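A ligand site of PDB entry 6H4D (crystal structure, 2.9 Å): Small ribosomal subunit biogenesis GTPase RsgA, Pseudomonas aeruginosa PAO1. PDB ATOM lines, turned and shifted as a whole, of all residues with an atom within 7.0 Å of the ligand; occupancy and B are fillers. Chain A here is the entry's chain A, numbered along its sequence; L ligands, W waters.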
ATOM      1  N   VAL A 128       1.500  14.148  28.793  1.00  0.00           N
ATOM      2  CA  VAL A 128       2.814  13.713  29.247  1.00  0.00           C
ATOM      3  C   VAL A 128       3.960  14.588  28.751  1.00  0.00           C
ATOM      4  O   VAL A 128       4.144  14.818  27.556  1.00  0.00           O
ATOM      5  CB  VAL A 128       3.107  12.253  28.809  1.00  0.00           C
ATOM      6  CG1 VAL A 128       4.485  11.833  29.289  1.00  0.00           C
ATOM      7  CG2 VAL A 128       2.053  11.341  29.373  1.00  0.00           C
ATOM      8  N   ALA A 130       8.258  15.877  30.172  1.00  0.00           N
ATOM      9  CA  ALA A 130       9.426  15.356  30.850  1.00  0.00           C
ATOM     10  C   ALA A 130      10.493  16.439  31.015  1.00  0.00           C
ATOM     11  O   ALA A 130      10.388  17.490  30.401  1.00  0.00           O
ATOM     12  CB  ALA A 130       9.974  14.168  30.083  1.00  0.00           C
ATOM     13  N   ARG A 132      13.436  16.213  29.806  1.00  0.00           N
ATOM     14  CA  ARG A 132      14.020  16.251  28.465  1.00  0.00           C
ATOM     15  C   ARG A 132      13.097  15.486  27.524  1.00  0.00           C
ATOM     16  O   ARG A 132      12.784  14.330  27.775  1.00  0.00           O
ATOM     17  CB  ARG A 132      15.433  15.655  28.461  1.00  0.00           C
ATOM     18  CG  ARG A 132      16.087  15.521  27.089  1.00  0.00           C
ATOM     19  CD  ARG A 132      17.536  15.018  27.184  1.00  0.00           C
ATOM     20  NE  ARG A 132      17.645  13.678  27.776  1.00  0.00           N
ATOM     21  CZ  ARG A 132      18.192  12.631  27.174  1.00  0.00           C
ATOM     22  NH1 ARG A 132      18.699  12.753  25.950  1.00  0.00           N
ATOM     23  NH2 ARG A 132      18.247  11.464  27.787  1.00  0.00           N
ATOM     24  N   PRO A 133      12.630  16.131  26.444  1.00  0.00           N
ATOM     25  CA  PRO A 133      12.950  17.506  26.045  1.00  0.00           C
ATOM     26  C   PRO A 133      12.261  18.533  26.941  1.00  0.00           C
ATOM     27  O   PRO A 133      11.263  18.179  27.579  1.00  0.00           O
ATOM     28  CB  PRO A 133      12.417  17.582  24.606  1.00  0.00           C
ATOM     29  CG  PRO A 133      11.660  16.309  24.369  1.00  0.00           C
ATOM     30  CD  PRO A 133      11.522  15.585  25.641  1.00  0.00           C
ATOM     31  N   ASN A 159       6.851  12.571  33.148  1.00  0.00           N
ATOM     32  CA  ASN A 159       7.625  11.374  32.865  1.00  0.00           C
ATOM     33  C   ASN A 159       9.112  11.686  33.010  1.00  0.00           C
ATOM     34  O   ASN A 159       9.510  12.854  33.072  1.00  0.00           O
ATOM     35  CB  ASN A 159       7.317  10.826  31.463  1.00  0.00           C
ATOM     36  CG  ASN A 159       7.963   9.483  31.215  1.00  0.00           C
ATOM     37  OD1 ASN A 159       8.353   8.782  32.162  1.00  0.00           O
ATOM     38  ND2 ASN A 159       8.104   9.113  29.946  1.00  0.00           N
ATOM     39  N   LYS A 160       9.933  10.634  33.047  1.00  0.00           N
ATOM     40  CA  LYS A 160      11.371  10.765  33.192  1.00  0.00           C
ATOM     41  C   LYS A 160      11.720  11.518  34.472  1.00  0.00           C
ATOM     42  O   LYS A 160      12.497  12.467  34.446  1.00  0.00           O
ATOM     43  CB  LYS A 160      11.984  11.482  31.989  1.00  0.00           C
ATOM     44  CG  LYS A 160      11.548  10.974  30.613  1.00  0.00           C
ATOM     45  CD  LYS A 160      12.456  11.527  29.516  1.00  0.00           C
ATOM     46  CE  LYS A 160      11.987  11.118  28.138  1.00  0.00           C
ATOM     47  NZ  LYS A 160      13.020  11.432  27.092  1.00  0.00           N
ATOM     48  N   ALA A 161      11.142  11.088  35.591  1.00  0.00           N
ATOM     49  CA  ALA A 161      11.399  11.744  36.864  1.00  0.00           C
ATOM     50  C   ALA A 161      12.767  11.332  37.401  1.00  0.00           C
ATOM     51  O   ALA A 161      13.313  11.973  38.302  1.00  0.00           O
ATOM     52  CB  ALA A 161      10.324  11.416  37.878  1.00  0.00           C
ATOM     53  N   ASP A 162      13.304  10.247  36.830  1.00  0.00           N
ATOM     54  CA  ASP A 162      14.645   9.781  37.155  1.00  0.00           C
ATOM     55  C   ASP A 162      15.708  10.788  36.733  1.00  0.00           C
ATOM     56  O   ASP A 162      16.847  10.713  37.177  1.00  0.00           O
ATOM     57  CB  ASP A 162      14.934   8.434  36.493  1.00  0.00           C
ATOM     58  CG  ASP A 162      14.670   8.445  34.994  1.00  0.00           C
ATOM     59  OD1 ASP A 162      13.531   8.772  34.593  1.00  0.00           O
ATOM     60  OD2 ASP A 162      15.597   8.167  34.216  1.00  0.00           O
ATOM     61  N   LEU A 163      15.306  11.729  35.891  1.00  0.00           N
ATOM     62  CA  LEU A 163      16.220  12.756  35.379  1.00  0.00           C
ATOM     63  C   LEU A 163      16.103  14.099  36.126  1.00  0.00           C
ATOM     64  O   LEU A 163      16.668  15.100  35.694  1.00  0.00           O
ATOM     65  CB  LEU A 163      15.975  12.953  33.877  1.00  0.00           C
ATOM     66  CG  LEU A 163      17.047  12.348  32.957  1.00  0.00           C
ATOM     67  CD1 LEU A 163      17.368  10.923  33.360  1.00  0.00           C
ATOM     68  CD2 LEU A 163      16.620  12.404  31.494  1.00  0.00           C
ATOM     69  N   VAL A 189       6.644  10.470  37.330  1.00  0.00           N
ATOM     70  CA  VAL A 189       6.914   9.055  37.093  1.00  0.00           C
ATOM     71  C   VAL A 189       8.180   8.785  36.290  1.00  0.00           C
ATOM     72  O   VAL A 189       8.756   9.694  35.692  1.00  0.00           O
ATOM     73  CB  VAL A 189       5.765   8.374  36.351  1.00  0.00           C
ATOM     74  CG1 VAL A 189       4.495   8.407  37.181  1.00  0.00           C
ATOM     75  CG2 VAL A 189       5.551   9.069  35.022  1.00  0.00           C
ATOM     76  N   SER A 190       8.582   7.523  36.263  1.00  0.00           N
ATOM     77  CA  SER A 190       9.613   7.070  35.360  1.00  0.00           C
ATOM     78  C   SER A 190       9.275   5.719  34.746  1.00  0.00           C
ATOM     79  O   SER A 190       9.239   4.709  35.449  1.00  0.00           O
ATOM     80  CB  SER A 190      10.958   6.961  36.081  1.00  0.00           C
ATOM     81  OG  SER A 190      11.904   6.313  35.246  1.00  0.00           O
ATOM     82  N   ALA A 191       9.040   5.708  33.430  1.00  0.00           N
ATOM     83  CA  ALA A 191       8.913   4.457  32.702  1.00  0.00           C
ATOM     84  C   ALA A 191      10.271   3.780  32.539  1.00  0.00           C
ATOM     85  O   ALA A 191      10.368   2.717  31.914  1.00  0.00           O
ATOM     86  CB  ALA A 191       8.287   4.697  31.359  1.00  0.00           C
ATOM     87  N   PHE A 192      11.323   4.388  33.086  1.00  0.00           N
ATOM     88  CA  PHE A 192      12.652   3.768  33.139  1.00  0.00           C
ATOM     89  C   PHE A 192      12.852   3.071  34.478  1.00  0.00           C
ATOM     90  O   PHE A 192      13.101   1.859  34.514  1.00  0.00           O
ATOM     91  CB  PHE A 192      13.755   4.797  32.894  1.00  0.00           C
ATOM     92  CG  PHE A 192      15.148   4.212  32.830  1.00  0.00           C
ATOM     93  CD1 PHE A 192      15.511   3.340  31.824  1.00  0.00           C
ATOM     94  CD2 PHE A 192      16.105   4.574  33.762  1.00  0.00           C
ATOM     95  CE1 PHE A 192      16.794   2.827  31.765  1.00  0.00           C
ATOM     96  CE2 PHE A 192      17.378   4.061  33.700  1.00  0.00           C
ATOM     97  CZ  PHE A 192      17.727   3.188  32.703  1.00  0.00           C
ATOM     98  N   ASN A 193      12.741   3.843  35.560  1.00  0.00           N
ATOM     99  CA  ASN A 193      12.807   3.335  36.931  1.00  0.00           C
ATOM    100  C   ASN A 193      11.661   2.382  37.259  1.00  0.00           C
ATOM    101  O   ASN A 193      11.877   1.253  37.694  1.00  0.00           O
ATOM    102  CB  ASN A 193      12.762   4.472  37.955  1.00  0.00           C
ATOM    103  CG  ASN A 193      14.029   5.293  37.999  1.00  0.00           C
ATOM    104  OD1 ASN A 193      14.936   5.118  37.179  1.00  0.00           O
ATOM    105  ND2 ASN A 193      14.106   6.200  38.967  1.00  0.00           N
ATOM    106  N   GLY A 194      10.452   2.886  37.064  1.00  0.00           N
ATOM    107  CA  GLY A 194       9.246   2.234  37.562  1.00  0.00           C
ATOM    108  C   GLY A 194       8.645   3.099  38.662  1.00  0.00           C
ATOM    109  O   GLY A 194       7.614   2.762  39.244  1.00  0.00           O
ATOM    110  N   GLY A 213       1.058  14.108  24.138  1.00  0.00           N
ATOM    111  CA  GLY A 213       2.204  14.928  24.507  1.00  0.00           C
ATOM    112  C   GLY A 213       3.185  15.107  23.351  1.00  0.00           C
ATOM    113  O   GLY A 213       3.120  14.379  22.369  1.00  0.00           O
ATOM    114  N   GLN A 214       4.091  16.079  23.467  1.00  0.00           N
ATOM    115  CA  GLN A 214       5.132  16.296  22.466  1.00  0.00           C
ATOM    116  C   GLN A 214       5.939  15.029  22.270  1.00  0.00           C
ATOM    117  O   GLN A 214       6.042  14.215  23.190  1.00  0.00           O
ATOM    118  CB  GLN A 214       6.035  17.468  22.890  1.00  0.00           C
ATOM    119  CG  GLN A 214       6.817  17.208  24.159  1.00  0.00           C
ATOM    120  CD  GLN A 214       7.065  18.457  24.993  1.00  0.00           C
ATOM    121  OE1 GLN A 214       6.652  18.530  26.152  1.00  0.00           O
ATOM    122  NE2 GLN A 214       7.761  19.436  24.410  1.00  0.00           N
ATOM    123  N   SER A 215       6.514  14.825  21.082  1.00  0.00           N
ATOM    124  CA  SER A 215       7.236  13.587  20.827  1.00  0.00           C
ATOM    125  C   SER A 215       8.534  13.538  21.644  1.00  0.00           C
ATOM    126  O   SER A 215       9.146  14.565  21.914  1.00  0.00           O
ATOM    127  CB  SER A 215       7.517  13.421  19.337  1.00  0.00           C
ATOM    128  OG  SER A 215       8.022  14.616  18.767  1.00  0.00           O
ATOM    129  N   GLY A 216       8.916  12.323  22.039  1.00  0.00           N
ATOM    130  CA  GLY A 216      10.106  12.134  22.838  1.00  0.00           C
ATOM    131  C   GLY A 216       9.956  12.305  24.348  1.00  0.00           C
ATOM    132  O   GLY A 216      10.979  12.459  25.031  1.00  0.00           O
ATOM    133  N   VAL A 217       8.727  12.283  24.868  1.00  0.00           N
ATOM    134  CA  VAL A 217       8.523  12.342  26.330  1.00  0.00           C
ATOM    135  C   VAL A 217       8.296  10.974  26.938  1.00  0.00           C
ATOM    136  O   VAL A 217       8.226  10.841  28.163  1.00  0.00           O
ATOM    137  CB  VAL A 217       7.335  13.242  26.738  1.00  0.00           C
ATOM    138  CG1 VAL A 217       7.634  14.706  26.448  1.00  0.00           C
ATOM    139  CG2 VAL A 217       6.054  12.768  26.053  1.00  0.00           C
ATOM    140  N   GLY A 218       8.154   9.960  26.093  1.00  0.00           N
ATOM    141  CA  GLY A 218       8.052   8.583  26.564  1.00  0.00           C
ATOM    142  C   GLY A 218       6.679   7.952  26.480  1.00  0.00           C
ATOM    143  O   GLY A 218       6.387   7.023  27.233  1.00  0.00           O
ATOM    144  N   LYS A 219       5.859   8.450  25.556  1.00  0.00           N
ATOM    145  CA  LYS A 219       4.492   7.933  25.388  1.00  0.00           C
ATOM    146  C   LYS A 219       4.518   6.461  25.010  1.00  0.00           C
ATOM    147  O   LYS A 219       3.793   5.650  25.600  1.00  0.00           O
ATOM    148  CB  LYS A 219       3.733   8.744  24.339  1.00  0.00           C
ATOM    149  CG  LYS A 219       3.467  10.199  24.763  1.00  0.00           C
ATOM    150  CD  LYS A 219       2.760  10.982  23.661  1.00  0.00           C
ATOM    151  CE  LYS A 219       3.558  11.055  22.373  1.00  0.00           C
ATOM    152  NZ  LYS A 219       4.841  11.774  22.525  1.00  0.00           N
ATOM    153  N   SER A 220       5.357   6.110  24.039  1.00  0.00           N
ATOM    154  CA  SER A 220       5.487   4.715  23.662  1.00  0.00           C
ATOM    155  C   SER A 220       5.989   3.872  24.832  1.00  0.00           C
ATOM    156  O   SER A 220       5.427   2.817  25.146  1.00  0.00           O
ATOM    157  CB  SER A 220       6.419   4.574  22.461  1.00  0.00           C
ATOM    158  OG  SER A 220       5.883   5.255  21.336  1.00  0.00           O
ATOM    159  N   SER A 221       7.046   4.356  25.489  1.00  0.00           N
ATOM    160  CA  SER A 221       7.667   3.666  26.614  1.00  0.00           C
ATOM    161  C   SER A 221       6.691   3.439  27.758  1.00  0.00           C
ATOM    162  O   SER A 221       6.784   2.442  28.488  1.00  0.00           O
ATOM    163  CB  SER A 221       8.870   4.471  27.116  1.00  0.00           C
ATOM    164  OG  SER A 221       9.563   5.083  26.022  1.00  0.00           O
ATOM    165  N   LEU A 222       5.763   4.382  27.927  1.00  0.00           N
ATOM    166  CA  LEU A 222       4.781   4.326  28.990  1.00  0.00           C
ATOM    167  C   LEU A 222       3.673   3.301  28.703  1.00  0.00           C
ATOM    168  O   LEU A 222       3.327   2.487  29.570  1.00  0.00           O
ATOM    169  CB  LEU A 222       4.189   5.717  29.203  1.00  0.00           C
ATOM    170  CG  LEU A 222       4.848   6.629  30.243  1.00  0.00           C
ATOM    171  CD1 LEU A 222       4.368   8.073  30.094  1.00  0.00           C
ATOM    172  CD2 LEU A 222       4.556   6.132  31.658  1.00  0.00           C
ATOM    173  N   ARG A 269      -1.890  10.390  19.276  1.00  0.00           N
ATOM    174  CA  ARG A 269      -0.687  10.830  19.974  1.00  0.00           C
ATOM    175  C   ARG A 269      -0.297  12.244  19.583  1.00  0.00           C
ATOM    176  O   ARG A 269       0.236  12.991  20.399  1.00  0.00           O
ATOM    177  CB  ARG A 269       0.468   9.875  19.683  1.00  0.00           C
ATOM    178  CG  ARG A 269       0.209   8.433  20.067  1.00  0.00           C
ATOM    179  CD  ARG A 269       0.612   8.138  21.495  1.00  0.00           C
ATOM    180  NE  ARG A 269       0.629   6.695  21.739  1.00  0.00           N
ATOM    181  CZ  ARG A 269       1.689   5.913  21.523  1.00  0.00           C
ATOM    182  NH1 ARG A 269       2.825   6.443  21.076  1.00  0.00           N
ATOM    183  NH2 ARG A 269       1.615   4.615  21.771  1.00  0.00           N
HETATM  184  P1  LIG L   1       7.601   9.288  22.404  1.00  0.00           P
HETATM  185  O1  LIG L   1       6.764   8.062  22.150  1.00  0.00           O
HETATM  186  O2  LIG L   1       8.038   9.939  21.106  1.00  0.00           O
HETATM  187  O3  LIG L   1       6.811  10.304  23.200  1.00  0.00           O
HETATM  188  O4  LIG L   1       8.907   8.910  23.248  1.00  0.00           O
HETATM  189  P2  LIG L   1       9.475   7.414  23.394  1.00  0.00           P
HETATM  190  O5  LIG L   1       9.824   6.829  22.034  1.00  0.00           O
HETATM  191  O6  LIG L   1       8.533   6.513  24.144  1.00  0.00           O
HETATM  192  O7  LIG L   1      10.789   7.696  24.260  1.00  0.00           O
HETATM  193  C1  LIG L   1      11.760   8.606  23.748  1.00  0.00           C
HETATM  194  C2  LIG L   1      12.997   8.485  24.617  1.00  0.00           C
HETATM  195  O8  LIG L   1      12.650   8.773  25.960  1.00  0.00           O
HETATM  196  C3  LIG L   1      13.470   7.043  24.582  1.00  0.00           C
HETATM  197  O9  LIG L   1      14.844   7.012  24.193  1.00  0.00           O
HETATM  198  C4  LIG L   1      13.317   6.511  25.999  1.00  0.00           C
HETATM  199  O10 LIG L   1      14.431   5.734  26.410  1.00  0.00           O
HETATM  200  C5  LIG L   1      13.227   7.777  26.823  1.00  0.00           C
HETATM  201  N1  LIG L   1      12.454   7.580  28.077  1.00  0.00           N
HETATM  202  C6  LIG L   1      11.176   7.203  28.237  1.00  0.00           C
HETATM  203  N2  LIG L   1      10.863   7.161  29.565  1.00  0.00           N
HETATM  204  C7  LIG L   1      11.940   7.529  30.261  1.00  0.00           C
HETATM  205  C8  LIG L   1      12.304   7.702  31.680  1.00  0.00           C
HETATM  206  O11 LIG L   1      11.489   7.484  32.590  1.00  0.00           O
HETATM  207  N3  LIG L   1      13.563   8.112  31.941  1.00  0.00           N
HETATM  208  C9  LIG L   1      14.469   8.361  30.985  1.00  0.00           C
HETATM  209  N4  LIG L   1      15.709   8.763  31.328  1.00  0.00           N
HETATM  210  N5  LIG L   1      14.194   8.220  29.670  1.00  0.00           N
HETATM  211  C10 LIG L   1      12.977   7.803  29.265  1.00  0.00           C
HETATM  212  O   HOH W   1      15.503   9.987  26.906  1.00  0.00           O
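Water W1 lies within hydrogen-bond range of the side-chain amino group (NZ) of Lys 160 (2.9 Å), the guanidinium group (NH2) of Arg 132 (3.2 Å) and an oxygen (O8) of the ligand (3.2 Å).
Merely in contact with the ligand: Leu 163, Gln 214 and Ser 215.
Hydrophobic or aromatic side chains that line the ligand: Leu 163, Ala 191, Phe 192 and Val 217.
An oxygen (O3) of the ligand lies within hydrogen-bond range of the backbone NH of Lys 219 (3.1 Å).
NZ of Lys 219 is in salt-bridge range of O3 of the ligand (2.5 Å).
The backbone NH (N) of Ser 221 lies within hydrogen-bond range of an oxygen (O6) of the ligand (2.9 Å).
The side-chain hydroxyl (OG) of Ser 221 lies within hydrogen-bond range of an oxygen (O6) of the ligand, at 2.6 Å.
N of Gly 216 lies within hydrogen-bond range of O2 of the ligand (2.7 Å).
The side-chain carboxylate of Asp 162 lies within hydrogen-bond range of a nitrogen (N3) of the ligand (2.7 Å).
The side-chain amino group (NZ) of Lys 160 sits at hydrogen-bond distance from an oxygen (O8) of the ligand.
An oxygen (O11) of the ligand lies within hydrogen-bond range of the side-chain hydroxyl of Ser 190 (2.9 Å).
N of Ser 220 is in hydrogen-bond range of O1 of the ligand (3.1 Å).
OG of Ser 220 sits at hydrogen-bond distance from O1 of the ligand, 3.1 Å away.
The backbone NH (N) of Gly 218 sits at hydrogen-bond distance from an oxygen (O4) of the ligand, 3.1 Å away.
N of Phe 192 lies within hydrogen-bond range of O11 of the ligand (3.1 Å).
N of Ala 191 lies within hydrogen-bond range of O11 of the ligand (3.1 Å).
An oxygen (O3) of the ligand sits at hydrogen-bond distance from the backbone NH (N) of Val 217, 3.2 Å away.
N2 of the ligand lies within hydrogen-bond range of ND2 of Asn 159 (3.4 Å).
The side-chain amino group of Lys 219 lies within hydrogen-bond range of the backbone carbonyl oxygen of Gln 214.
The side-chain amino group of Lys 219 sits at hydrogen-bond distance from the backbone carbonyl oxygen of Gly 213, at 3.1 Å.
O of Gly 216 is in hydrogen-bond range of NZ of Lys 160, at 3.1 Å.
The backbone NH (N) of Lys 160 lies within hydrogen-bond range of the backbone carbonyl oxygen (O) of Val 189 (3.0 Å).
The backbone carbonyl oxygen (O) of Arg 132 sits at hydrogen-bond distance from the side-chain amino group (NZ) of Lys 160 (3.0 Å).
The side-chain hydroxyl (OG) of Ser 190 lies within hydrogen-bond range of the backbone NH (N) of Phe 192 (3.0 Å).
The backbone NH (N) of Ala 191 lies within hydrogen-bond range of the side-chain amide oxygen (OD1) of Asn 159 (3.4 Å).
The side-chain amide nitrogen of Asn 159 is in hydrogen-bond range of the backbone carbonyl oxygen of Val 217, at 2.5 Å.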
